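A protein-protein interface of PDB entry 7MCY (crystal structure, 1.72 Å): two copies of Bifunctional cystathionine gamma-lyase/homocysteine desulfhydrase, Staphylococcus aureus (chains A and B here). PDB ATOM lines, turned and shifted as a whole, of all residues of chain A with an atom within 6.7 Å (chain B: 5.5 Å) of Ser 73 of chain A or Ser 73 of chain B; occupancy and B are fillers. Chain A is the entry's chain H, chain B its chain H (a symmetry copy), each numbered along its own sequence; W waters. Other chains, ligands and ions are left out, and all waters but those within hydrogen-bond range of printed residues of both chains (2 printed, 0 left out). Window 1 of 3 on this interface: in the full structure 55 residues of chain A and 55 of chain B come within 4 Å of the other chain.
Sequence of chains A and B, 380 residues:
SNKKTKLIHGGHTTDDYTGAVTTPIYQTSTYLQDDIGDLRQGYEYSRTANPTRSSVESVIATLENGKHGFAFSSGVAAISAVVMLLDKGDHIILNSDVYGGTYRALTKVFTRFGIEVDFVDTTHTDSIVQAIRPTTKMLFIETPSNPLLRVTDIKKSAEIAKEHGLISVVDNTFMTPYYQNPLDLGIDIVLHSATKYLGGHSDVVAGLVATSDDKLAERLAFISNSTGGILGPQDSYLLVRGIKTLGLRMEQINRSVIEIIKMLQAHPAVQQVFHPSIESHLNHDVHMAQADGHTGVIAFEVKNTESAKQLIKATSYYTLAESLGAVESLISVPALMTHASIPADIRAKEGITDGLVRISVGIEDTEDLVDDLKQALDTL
Ser 73 of chain B touches its own counterpart, Ser 73 of chain A.
Ser 73 of chain A touches Gly 229 of chain B, and with the chains exchanged Gly 229 of chain A touches Ser 73 of chain B.
Ser 73 of chain A touches Ile 230 of chain B, and with the chains exchanged Ile 230 of chain A touches Ser 73 of chain B.
Ser 74 of chain A touches Gly 228 of chain B, and with the chains exchanged Gly 228 of chain A touches Ser 74 of chain B.
Positions printed for both chains: 71, 72, 73, 74, 75, 77, 205, 206, 207, 228, 229, 230 and 231.
The backbone carbonyl oxygen (O) of Gly 228 of chain A lies within hydrogen-bond range of the side-chain hydroxyl (OG) of Ser 74 of chain B (2.8 Å).
O of Thr 227 of chain A lies close to N of Ala 77 of chain B, at 3.4 Å.
The side-chain hydroxyl of Ser 73 of chain A lies within hydrogen-bond range of the backbone carbonyl oxygen of Gly 228 of chain B (2.8 Å).
O of Gly 228 of chain A is in hydrogen-bond range of OG of Ser 73 of chain B, 2.8 Å away.
The side-chain hydroxyl of Ser 74 of chain A lies within hydrogen-bond range of the backbone carbonyl oxygen of Gly 228 of chain B.
Of the printed residues of chain B, Ser 73 of chain A touches Ser 73 (3.8 Å), Gly 228 (2.8 Å), Gly 229 (3.3 Å) and Ile 230 (3.5 Å).
Ser 73 of chain B touches just these residues of chain A: Ser 73 (3.8 Å), Gly 228 (2.8 Å), Gly 229 (3.3 Å) and Ile 230 (3.5 Å).
Printed residues of chain A within 4 Å of Ser 74 of chain B: Gly 228 (2.8 Å).
Of the printed residues of chain B, Gly 228 of chain A touches Ser 73, Ser 74 and Ala 77.
Printed residues of chain B within 4 Å of Thr 227 of chain A: Ala 77 (3.1 Å).
Of the printed residues of chain B, Gly 229 of chain A touches Ser 73.
Of the printed residues of chain B, Val 76 of chain A touches Gly 228.
Gly 207 of chain A touches none of the printed residues of chain B.
LLP 196 of chain A touches none of the printed residues of chain B.
The nearest printed residue of chain B that does not touch Ser 73 of chain A is Leu 231 of chain B (5.7 Å).
The nearest residue of chain A that does not touch Ser 73 of chain B is Thr 227 of chain A (5.6 Å).
Ser 73 of chain A touches Ser 73 of chain B.
Ser 73 of chain A touches Gly 229 of chain B (OG to CA, 3.3 Å).
CB of Ser 73 of chain A touches O of Ile 230 of chain B (3.5 Å).
Val 76 of chain A touches Gly 228 of chain B (CG2 to CA, 3.6 Å).
Ala 77 of chain A touches Gly 228 of chain B (CB to O, 3.5 Å).
CB of Ala 77 of chain B touches O of Gly 228 of chain A, 3.5 Å away.
CA of Gly 229 of chain A touches OG of Ser 73 of chain B, at 3.3 Å.
Ser 73 of chain B touches Ile 230 of chain A.
N of Ala 77 of chain A sits at hydrogen-bond distance from OG of Ser 74 of chain A, at 3.0 Å.
The backbone NH of Ser 73 of chain B lies within hydrogen-bond range of the backbone carbonyl oxygen of Gly 229 of chain B (2.9 Å).
OP3 of LLP 196 of chain A lies within hydrogen-bond range of the backbone NH (N) of Val 76 of chain A (2.8 Å).
The backbone carbonyl oxygen (O) of Ser 74 of chain A lies close to the backbone NH (N) of Gly 207 of chain A (3.3 Å).
O of Ser 74 of chain B lies close to N of Gly 207 of chain B (3.3 Å).
The side-chain hydroxyl of Ser 74 of chain B sits at hydrogen-bond distance from the backbone NH of Ala 77 of chain B.
Water W1 bridges O of Ile 230 of chain A and O of Ser 73 of chain B.
Water W2 bridges O of Ile 230 of chain B and O of Ser 73 of chain A.
Hydrophobic or aromatic side chains of chain B that line the printed part of chain A: Ala 77 and Ile 230.
Hydrophobic or aromatic side chains of chain A that line the printed part of chain B: Val 76, Ala 77 and Ile 230.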
ATOM      1  N   ARG A  47      20.657  -2.356 -23.877  1.00  0.00           N
ATOM      2  CA  ARG A  47      19.445  -3.149 -24.097  1.00  0.00           C
ATOM      3  C   ARG A  47      19.810  -4.527 -24.631  1.00  0.00           C
ATOM      4  O   ARG A  47      19.280  -5.548 -24.172  1.00  0.00           O
ATOM      5  CB  ARG A  47      18.475  -2.445 -25.051  1.00  0.00           C
ATOM      6  CG  ARG A  47      17.405  -3.410 -25.587  1.00  0.00           C
ATOM      7  CD  ARG A  47      16.132  -2.726 -26.059  1.00  0.00           C
ATOM      8  NE  ARG A  47      16.346  -1.553 -26.902  1.00  0.00           N
ATOM      9  CZ  ARG A  47      16.770  -1.580 -28.159  1.00  0.00           C
ATOM     10  NH1 ARG A  47      17.034  -2.739 -28.756  1.00  0.00           N
ATOM     11  NH2 ARG A  47      16.931  -0.439 -28.822  1.00  0.00           N
ATOM     12  N   ALA A  71      17.605 -12.146 -18.162  1.00  0.00           N
ATOM     13  CA  ALA A  71      17.058 -11.375 -17.053  1.00  0.00           C
ATOM     14  C   ALA A  71      16.082 -10.330 -17.577  1.00  0.00           C
ATOM     15  O   ALA A  71      16.427  -9.529 -18.456  1.00  0.00           O
ATOM     16  CB  ALA A  71      18.176 -10.696 -16.244  1.00  0.00           C
ATOM     17  N   PHE A  72      14.870 -10.339 -17.031  1.00  0.00           N
ATOM     18  CA  PHE A  72      13.783  -9.475 -17.451  1.00  0.00           C
ATOM     19  C   PHE A  72      13.356  -8.573 -16.300  1.00  0.00           C
ATOM     20  O   PHE A  72      13.623  -8.856 -15.129  1.00  0.00           O
ATOM     21  CB  PHE A  72      12.582 -10.310 -17.931  1.00  0.00           C
ATOM     22  CG  PHE A  72      12.862 -11.104 -19.186  1.00  0.00           C
ATOM     23  CD1 PHE A  72      13.372 -12.393 -19.109  1.00  0.00           C
ATOM     24  CD2 PHE A  72      12.638 -10.548 -20.432  1.00  0.00           C
ATOM     25  CE1 PHE A  72      13.638 -13.124 -20.267  1.00  0.00           C
ATOM     26  CE2 PHE A  72      12.906 -11.270 -21.604  1.00  0.00           C
ATOM     27  CZ  PHE A  72      13.399 -12.560 -21.514  1.00  0.00           C
ATOM     28  N   SER A  73      12.642  -7.503 -16.652  1.00  0.00           N
ATOM     29  CA  SER A  73      12.219  -6.478 -15.705  1.00  0.00           C
ATOM     30  C   SER A  73      11.187  -6.965 -14.686  1.00  0.00           C
ATOM     31  O   SER A  73      10.887  -6.223 -13.742  1.00  0.00           O
ATOM     32  CB  SER A  73      11.652  -5.286 -16.480  1.00  0.00           C
ATOM     33  OG  SER A  73      10.748  -5.750 -17.477  1.00  0.00           O
ATOM     34  N   SER A  74      10.629  -8.166 -14.851  1.00  0.00           N
ATOM     35  CA  SER A  74       9.696  -8.749 -13.890  1.00  0.00           C
ATOM     36  C   SER A  74       9.480 -10.204 -14.284  1.00  0.00           C
ATOM     37  O   SER A  74       9.802 -10.617 -15.404  1.00  0.00           O
ATOM     38  CB  SER A  74       8.349  -8.018 -13.874  1.00  0.00           C
ATOM     39  OG  SER A  74       7.755  -8.079 -15.166  1.00  0.00           O
ATOM     40  N   GLY A  75       8.917 -10.975 -13.351  1.00  0.00           N
ATOM     41  CA  GLY A  75       8.478 -12.323 -13.695  1.00  0.00           C
ATOM     42  C   GLY A  75       7.493 -12.354 -14.855  1.00  0.00           C
ATOM     43  O   GLY A  75       7.604 -13.198 -15.757  1.00  0.00           O
ATOM     44  N   VAL A  76       6.512 -11.444 -14.861  1.00  0.00           N
ATOM     45  CA  VAL A  76       5.552 -11.521 -15.967  1.00  0.00           C
ATOM     46  C   VAL A  76       6.175 -11.058 -17.279  1.00  0.00           C
ATOM     47  O   VAL A  76       5.706 -11.459 -18.353  1.00  0.00           O
ATOM     48  CB  VAL A  76       4.245 -10.743 -15.698  1.00  0.00           C
ATOM     49  CG1 VAL A  76       3.481 -11.318 -14.495  1.00  0.00           C
ATOM     50  CG2 VAL A  76       4.496  -9.277 -15.529  1.00  0.00           C
ATOM     51  N   ALA A  77       7.235 -10.249 -17.242  1.00  0.00           N
ATOM     52  CA  ALA A  77       7.945  -9.942 -18.486  1.00  0.00           C
ATOM     53  C   ALA A  77       8.672 -11.172 -19.016  1.00  0.00           C
ATOM     54  O   ALA A  77       8.710 -11.397 -20.230  1.00  0.00           O
ATOM     55  CB  ALA A  77       8.922  -8.776 -18.280  1.00  0.00           C
ATOM     56  N   ALA A  78       9.239 -11.988 -18.123  1.00  0.00           N
ATOM     57  CA  ALA A  78       9.847 -13.248 -18.544  1.00  0.00           C
ATOM     58  C   ALA A  78       8.808 -14.164 -19.173  1.00  0.00           C
ATOM     59  O   ALA A  78       9.038 -14.765 -20.235  1.00  0.00           O
ATOM     60  CB  ALA A  78      10.505 -13.938 -17.351  1.00  0.00           C
ATOM     61  N   THR A 195      11.656 -11.847  -8.188  1.00  0.00           N
ATOM     62  CA  THR A 195      11.052 -10.982  -7.180  1.00  0.00           C
ATOM     63  C   THR A 195      10.874 -11.697  -5.840  1.00  0.00           C
ATOM     64  O   THR A 195      10.874 -11.066  -4.773  1.00  0.00           O
ATOM     65  CB  THR A 195       9.668 -10.485  -7.686  1.00  0.00           C
ATOM     66  OG1 THR A 195       9.816  -9.941  -9.004  1.00  0.00           O
ATOM     67  CG2 THR A 195       9.079  -9.426  -6.755  1.00  0.00           C
ATOM     68  N1  LLP A 196       4.937 -16.685 -11.198  1.00  0.00           N
ATOM     69  C2  LLP A 196       4.894 -16.948  -9.919  1.00  0.00           C
ATOM     70  C2' LLP A 196       4.802 -18.384  -9.507  1.00  0.00           C
ATOM     71  C3  LLP A 196       4.945 -15.926  -8.960  1.00  0.00           C
ATOM     72  O3  LLP A 196       4.897 -16.278  -7.610  1.00  0.00           O
ATOM     73  C4  LLP A 196       5.029 -14.594  -9.362  1.00  0.00           C
ATOM     74  C4' LLP A 196       5.113 -13.523  -8.329  1.00  0.00           C
ATOM     75  C5  LLP A 196       5.059 -14.338 -10.760  1.00  0.00           C
ATOM     76  C6  LLP A 196       5.014 -15.438 -11.605  1.00  0.00           C
ATOM     77  C5' LLP A 196       5.132 -12.946 -11.404  1.00  0.00           C
ATOM     78  OP4 LLP A 196       6.373 -12.349 -11.197  1.00  0.00           O
ATOM     79  P   LLP A 196       6.516 -10.734 -11.076  1.00  0.00           P
ATOM     80  OP1 LLP A 196       5.590 -10.283  -9.959  1.00  0.00           O
ATOM     81  OP2 LLP A 196       7.975 -10.499 -10.757  1.00  0.00           O
ATOM     82  OP3 LLP A 196       6.108 -10.137 -12.404  1.00  0.00           O
ATOM     83  N   LLP A 196      10.716 -13.020  -5.898  1.00  0.00           N
ATOM     84  CA  LLP A 196      10.389 -13.807  -4.712  1.00  0.00           C
ATOM     85  CB  LLP A 196       9.422 -14.950  -5.078  1.00  0.00           C
ATOM     86  CG  LLP A 196       8.327 -14.484  -6.049  1.00  0.00           C
ATOM     87  CD  LLP A 196       7.380 -13.451  -5.439  1.00  0.00           C
ATOM     88  CE  LLP A 196       6.475 -12.791  -6.513  1.00  0.00           C
ATOM     89  NZ  LLP A 196       5.506 -13.710  -7.105  1.00  0.00           N
ATOM     90  C   LLP A 196      11.688 -14.335  -4.074  1.00  0.00           C
ATOM     91  O   LLP A 196      12.536 -13.514  -3.650  1.00  0.00           O
ATOM     92  N   VAL A 205      12.128  -6.290  -8.314  1.00  0.00           N
ATOM     93  CA  VAL A 205      11.165  -6.948  -9.192  1.00  0.00           C
ATOM     94  C   VAL A 205      11.926  -7.391 -10.436  1.00  0.00           C
ATOM     95  O   VAL A 205      12.577  -6.571 -11.090  1.00  0.00           O
ATOM     96  CB  VAL A 205      10.001  -6.011  -9.554  1.00  0.00           C
ATOM     97  CG1 VAL A 205       9.069  -6.674 -10.580  1.00  0.00           C
ATOM     98  CG2 VAL A 205       9.231  -5.602  -8.286  1.00  0.00           C
ATOM     99  N   ALA A 206      11.853  -8.681 -10.767  1.00  0.00           N
ATOM    100  CA  ALA A 206      12.708  -9.221 -11.820  1.00  0.00           C
ATOM    101  C   ALA A 206      12.215 -10.600 -12.225  1.00  0.00           C
ATOM    102  O   ALA A 206      11.611 -11.317 -11.419  1.00  0.00           O
ATOM    103  CB  ALA A 206      14.172  -9.318 -11.350  1.00  0.00           C
ATOM    104  N   GLY A 207      12.503 -10.976 -13.471  1.00  0.00           N
ATOM    105  CA  GLY A 207      12.278 -12.332 -13.940  1.00  0.00           C
ATOM    106  C   GLY A 207      13.575 -12.917 -14.471  1.00  0.00           C
ATOM    107  O   GLY A 207      14.455 -12.191 -14.935  1.00  0.00           O
ATOM    108  N   THR A 227      11.548  -6.428 -27.826  1.00  0.00           N
ATOM    109  CA  THR A 227      10.479  -5.884 -26.994  1.00  0.00           C
ATOM    110  C   THR A 227      10.996  -5.284 -25.684  1.00  0.00           C
ATOM    111  O   THR A 227      10.238  -4.598 -24.993  1.00  0.00           O
ATOM    112  CB  THR A 227       9.421  -6.958 -26.710  1.00  0.00           C
ATOM    113  OG1 THR A 227      10.019  -8.081 -26.059  1.00  0.00           O
ATOM    114  CG2 THR A 227       8.784  -7.439 -28.033  1.00  0.00           C
ATOM    115  N   GLY A 228      12.251  -5.534 -25.326  1.00  0.00           N
ATOM    116  CA  GLY A 228      12.959  -4.648 -24.403  1.00  0.00           C
ATOM    117  C   GLY A 228      12.577  -4.703 -22.937  1.00  0.00           C
ATOM    118  O   GLY A 228      12.849  -3.738 -22.212  1.00  0.00           O
ATOM    119  N   GLY A 229      11.971  -5.795 -22.474  1.00  0.00           N
ATOM    120  CA  GLY A 229      11.669  -5.946 -21.057  1.00  0.00           C
ATOM    121  C   GLY A 229      12.867  -6.407 -20.241  1.00  0.00           C
ATOM    122  O   GLY A 229      12.790  -7.413 -19.538  1.00  0.00           O
ATOM    123  N   ILE A 230      13.982  -5.663 -20.306  1.00  0.00           N
ATOM    124  CA  ILE A 230      15.253  -6.097 -19.733  1.00  0.00           C
ATOM    125  C   ILE A 230      15.359  -5.630 -18.289  1.00  0.00           C
ATOM    126  O   ILE A 230      14.845  -4.572 -17.914  1.00  0.00           O
ATOM    127  CB  ILE A 230      16.435  -5.553 -20.562  1.00  0.00           C
ATOM    128  CG1 ILE A 230      16.340  -4.020 -20.620  1.00  0.00           C
ATOM    129  CG2 ILE A 230      16.400  -6.134 -21.973  1.00  0.00           C
ATOM    130  CD1 ILE A 230      17.650  -3.323 -20.730  1.00  0.00           C
ATOM    131  N   LEU A 231      16.059  -6.414 -17.479  1.00  0.00           N
ATOM    132  CA  LEU A 231      16.394  -6.000 -16.117  1.00  0.00           C
ATOM    133  C   LEU A 231      17.546  -5.001 -16.124  1.00  0.00           C
ATOM    134  O   LEU A 231      18.539  -5.187 -16.833  1.00  0.00           O
ATOM    135  CB  LEU A 231      16.768  -7.223 -15.275  1.00  0.00           C
ATOM    136  CG  LEU A 231      16.861  -6.974 -13.756  1.00  0.00           C
ATOM    137  CD1 LEU A 231      15.487  -6.555 -13.208  1.00  0.00           C
ATOM    138  CD2 LEU A 231      17.383  -8.215 -13.043  1.00  0.00           C
ATOM    139  N   GLY A 232      17.422  -3.944 -15.313  1.00  0.00           N
ATOM    140  CA  GLY A 232      18.474  -2.949 -15.187  1.00  0.00           C
ATOM    141  C   GLY A 232      19.662  -3.432 -14.371  1.00  0.00           C
ATOM    142  O   GLY A 232      19.598  -4.455 -13.682  1.00  0.00           O
ATOM    143  N   ALA B  71       6.478   4.600 -17.253  1.00  0.00           N
ATOM    144  CA  ALA B  71       7.909   4.363 -17.397  1.00  0.00           C
ATOM    145  C   ALA B  71       8.169   2.885 -17.655  1.00  0.00           C
ATOM    146  O   ALA B  71       7.723   2.023 -16.888  1.00  0.00           O
ATOM    147  CB  ALA B  71       8.677   4.826 -16.147  1.00  0.00           C
ATOM    148  N   PHE B  72       8.895   2.600 -18.731  1.00  0.00           N
ATOM    149  CA  PHE B  72       9.184   1.253 -19.184  1.00  0.00           C
ATOM    150  C   PHE B  72      10.686   1.002 -19.161  1.00  0.00           C
ATOM    151  O   PHE B  72      11.493   1.934 -19.159  1.00  0.00           O
ATOM    152  CB  PHE B  72       8.641   1.032 -20.608  1.00  0.00           C
ATOM    153  CG  PHE B  72       7.133   1.083 -20.694  1.00  0.00           C
ATOM    154  CD1 PHE B  72       6.478   2.285 -20.930  1.00  0.00           C
ATOM    155  CD2 PHE B  72       6.381  -0.064 -20.513  1.00  0.00           C
ATOM    156  CE1 PHE B  72       5.086   2.334 -21.002  1.00  0.00           C
ATOM    157  CE2 PHE B  72       4.981  -0.026 -20.578  1.00  0.00           C
ATOM    158  CZ  PHE B  72       4.340   1.174 -20.830  1.00  0.00           C
ATOM    159  N   SER B  73      11.047  -0.282 -19.193  1.00  0.00           N
ATOM    160  CA  SER B  73      12.433  -0.724 -19.089  1.00  0.00           C
ATOM    161  C   SER B  73      13.298  -0.339 -20.291  1.00  0.00           C
ATOM    162  O   SER B  73      14.521  -0.523 -20.228  1.00  0.00           O
ATOM    163  CB  SER B  73      12.459  -2.244 -18.905  1.00  0.00           C
ATOM    164  OG  SER B  73      11.587  -2.855 -19.849  1.00  0.00           O
ATOM    165  N   SER B  74      12.710   0.170 -21.376  1.00  0.00           N
ATOM    166  CA  SER B  74      13.459   0.641 -22.540  1.00  0.00           C
ATOM    167  C   SER B  74      12.482   1.373 -23.449  1.00  0.00           C
ATOM    168  O   SER B  74      11.260   1.242 -23.311  1.00  0.00           O
ATOM    169  CB  SER B  74      14.113  -0.510 -23.312  1.00  0.00           C
ATOM    170  OG  SER B  74      13.111  -1.415 -23.763  1.00  0.00           O
ATOM    171  N   GLY B  75      13.036   2.139 -24.391  1.00  0.00           N
ATOM    172  CA  GLY B  75      12.201   2.716 -25.438  1.00  0.00           C
ATOM    173  C   GLY B  75      11.411   1.673 -26.217  1.00  0.00           C
ATOM    174  O   GLY B  75      10.219   1.862 -26.497  1.00  0.00           O
ATOM    175  N   ALA B  77      10.426  -1.185 -25.187  1.00  0.00           N
ATOM    176  CA  ALA B  77       9.355  -1.710 -24.338  1.00  0.00           C
ATOM    177  C   ALA B  77       8.162  -0.762 -24.318  1.00  0.00           C
ATOM    178  O   ALA B  77       7.011  -1.211 -24.319  1.00  0.00           O
ATOM    179  CB  ALA B  77       9.868  -1.974 -22.916  1.00  0.00           C
ATOM    180  N   VAL B 205      18.851   2.916 -19.572  1.00  0.00           N
ATOM    181  CA  VAL B 205      18.000   2.476 -20.674  1.00  0.00           C
ATOM    182  C   VAL B 205      16.562   2.511 -20.169  1.00  0.00           C
ATOM    183  O   VAL B 205      16.250   1.895 -19.145  1.00  0.00           O
ATOM    184  CB  VAL B 205      18.389   1.071 -21.159  1.00  0.00           C
ATOM    185  CG1 VAL B 205      17.403   0.573 -22.227  1.00  0.00           C
ATOM    186  CG2 VAL B 205      19.832   1.069 -21.691  1.00  0.00           C
ATOM    187  N   ALA B 206      15.686   3.226 -20.875  1.00  0.00           N
ATOM    188  CA  ALA B 206      14.345   3.471 -20.353  1.00  0.00           C
ATOM    189  C   ALA B 206      13.455   4.014 -21.458  1.00  0.00           C
ATOM    190  O   ALA B 206      13.935   4.656 -22.399  1.00  0.00           O
ATOM    191  CB  ALA B 206      14.380   4.476 -19.185  1.00  0.00           C
ATOM    192  N   GLY B 207      12.151   3.774 -21.322  1.00  0.00           N
ATOM    193  CA  GLY B 207      11.157   4.394 -22.183  1.00  0.00           C
ATOM    194  C   GLY B 207      10.144   5.151 -21.342  1.00  0.00           C
ATOM    195  O   GLY B 207       9.900   4.808 -20.184  1.00  0.00           O
ATOM    196  N   GLY B 228       4.661  -6.353 -17.922  1.00  0.00           N
ATOM    197  CA  GLY B 228       5.713  -6.173 -16.922  1.00  0.00           C
ATOM    198  C   GLY B 228       7.021  -5.557 -17.376  1.00  0.00           C
ATOM    199  O   GLY B 228       8.038  -5.744 -16.695  1.00  0.00           O
ATOM    200  N   GLY B 229       7.033  -4.826 -18.489  1.00  0.00           N
ATOM    201  CA  GLY B 229       8.236  -4.129 -18.921  1.00  0.00           C
ATOM    202  C   GLY B 229       8.453  -2.812 -18.192  1.00  0.00           C
ATOM    203  O   GLY B 229       8.594  -1.767 -18.825  1.00  0.00           O
ATOM    204  N   ILE B 230       8.506  -2.849 -16.852  1.00  0.00           N
ATOM    205  CA  ILE B 230       8.513  -1.641 -16.030  1.00  0.00           C
ATOM    206  C   ILE B 230       9.943  -1.179 -15.796  1.00  0.00           C
ATOM    207  O   ILE B 230      10.875  -1.984 -15.714  1.00  0.00           O
ATOM    208  CB  ILE B 230       7.804  -1.900 -14.684  1.00  0.00           C
ATOM    209  CG1 ILE B 230       8.501  -3.068 -13.968  1.00  0.00           C
ATOM    210  CG2 ILE B 230       6.332  -2.230 -14.918  1.00  0.00           C
ATOM    211  CD1 ILE B 230       8.450  -3.004 -12.483  1.00  0.00           C
ATOM    212  N   LEU B 231      10.111   0.130 -15.658  1.00  0.00           N
ATOM    213  CA  LEU B 231      11.395   0.697 -15.251  1.00  0.00           C
ATOM    214  C   LEU B 231      11.611   0.525 -13.751  1.00  0.00           C
ATOM    215  O   LEU B 231      10.700   0.761 -12.951  1.00  0.00           O
ATOM    216  CB  LEU B 231      11.454   2.181 -15.621  1.00  0.00           C
ATOM    217  CG  LEU B 231      12.848   2.832 -15.516  1.00  0.00           C
ATOM    218  CD1 LEU B 231      13.814   2.166 -16.509  1.00  0.00           C
ATOM    219  CD2 LEU B 231      12.756   4.332 -15.760  1.00  0.00           C
HETATM  220  O   HOH W   1      15.367  -1.831 -17.492  1.00  0.00           O
HETATM  221  O   HOH W   2      12.418  -3.475 -13.881  1.00  0.00           O
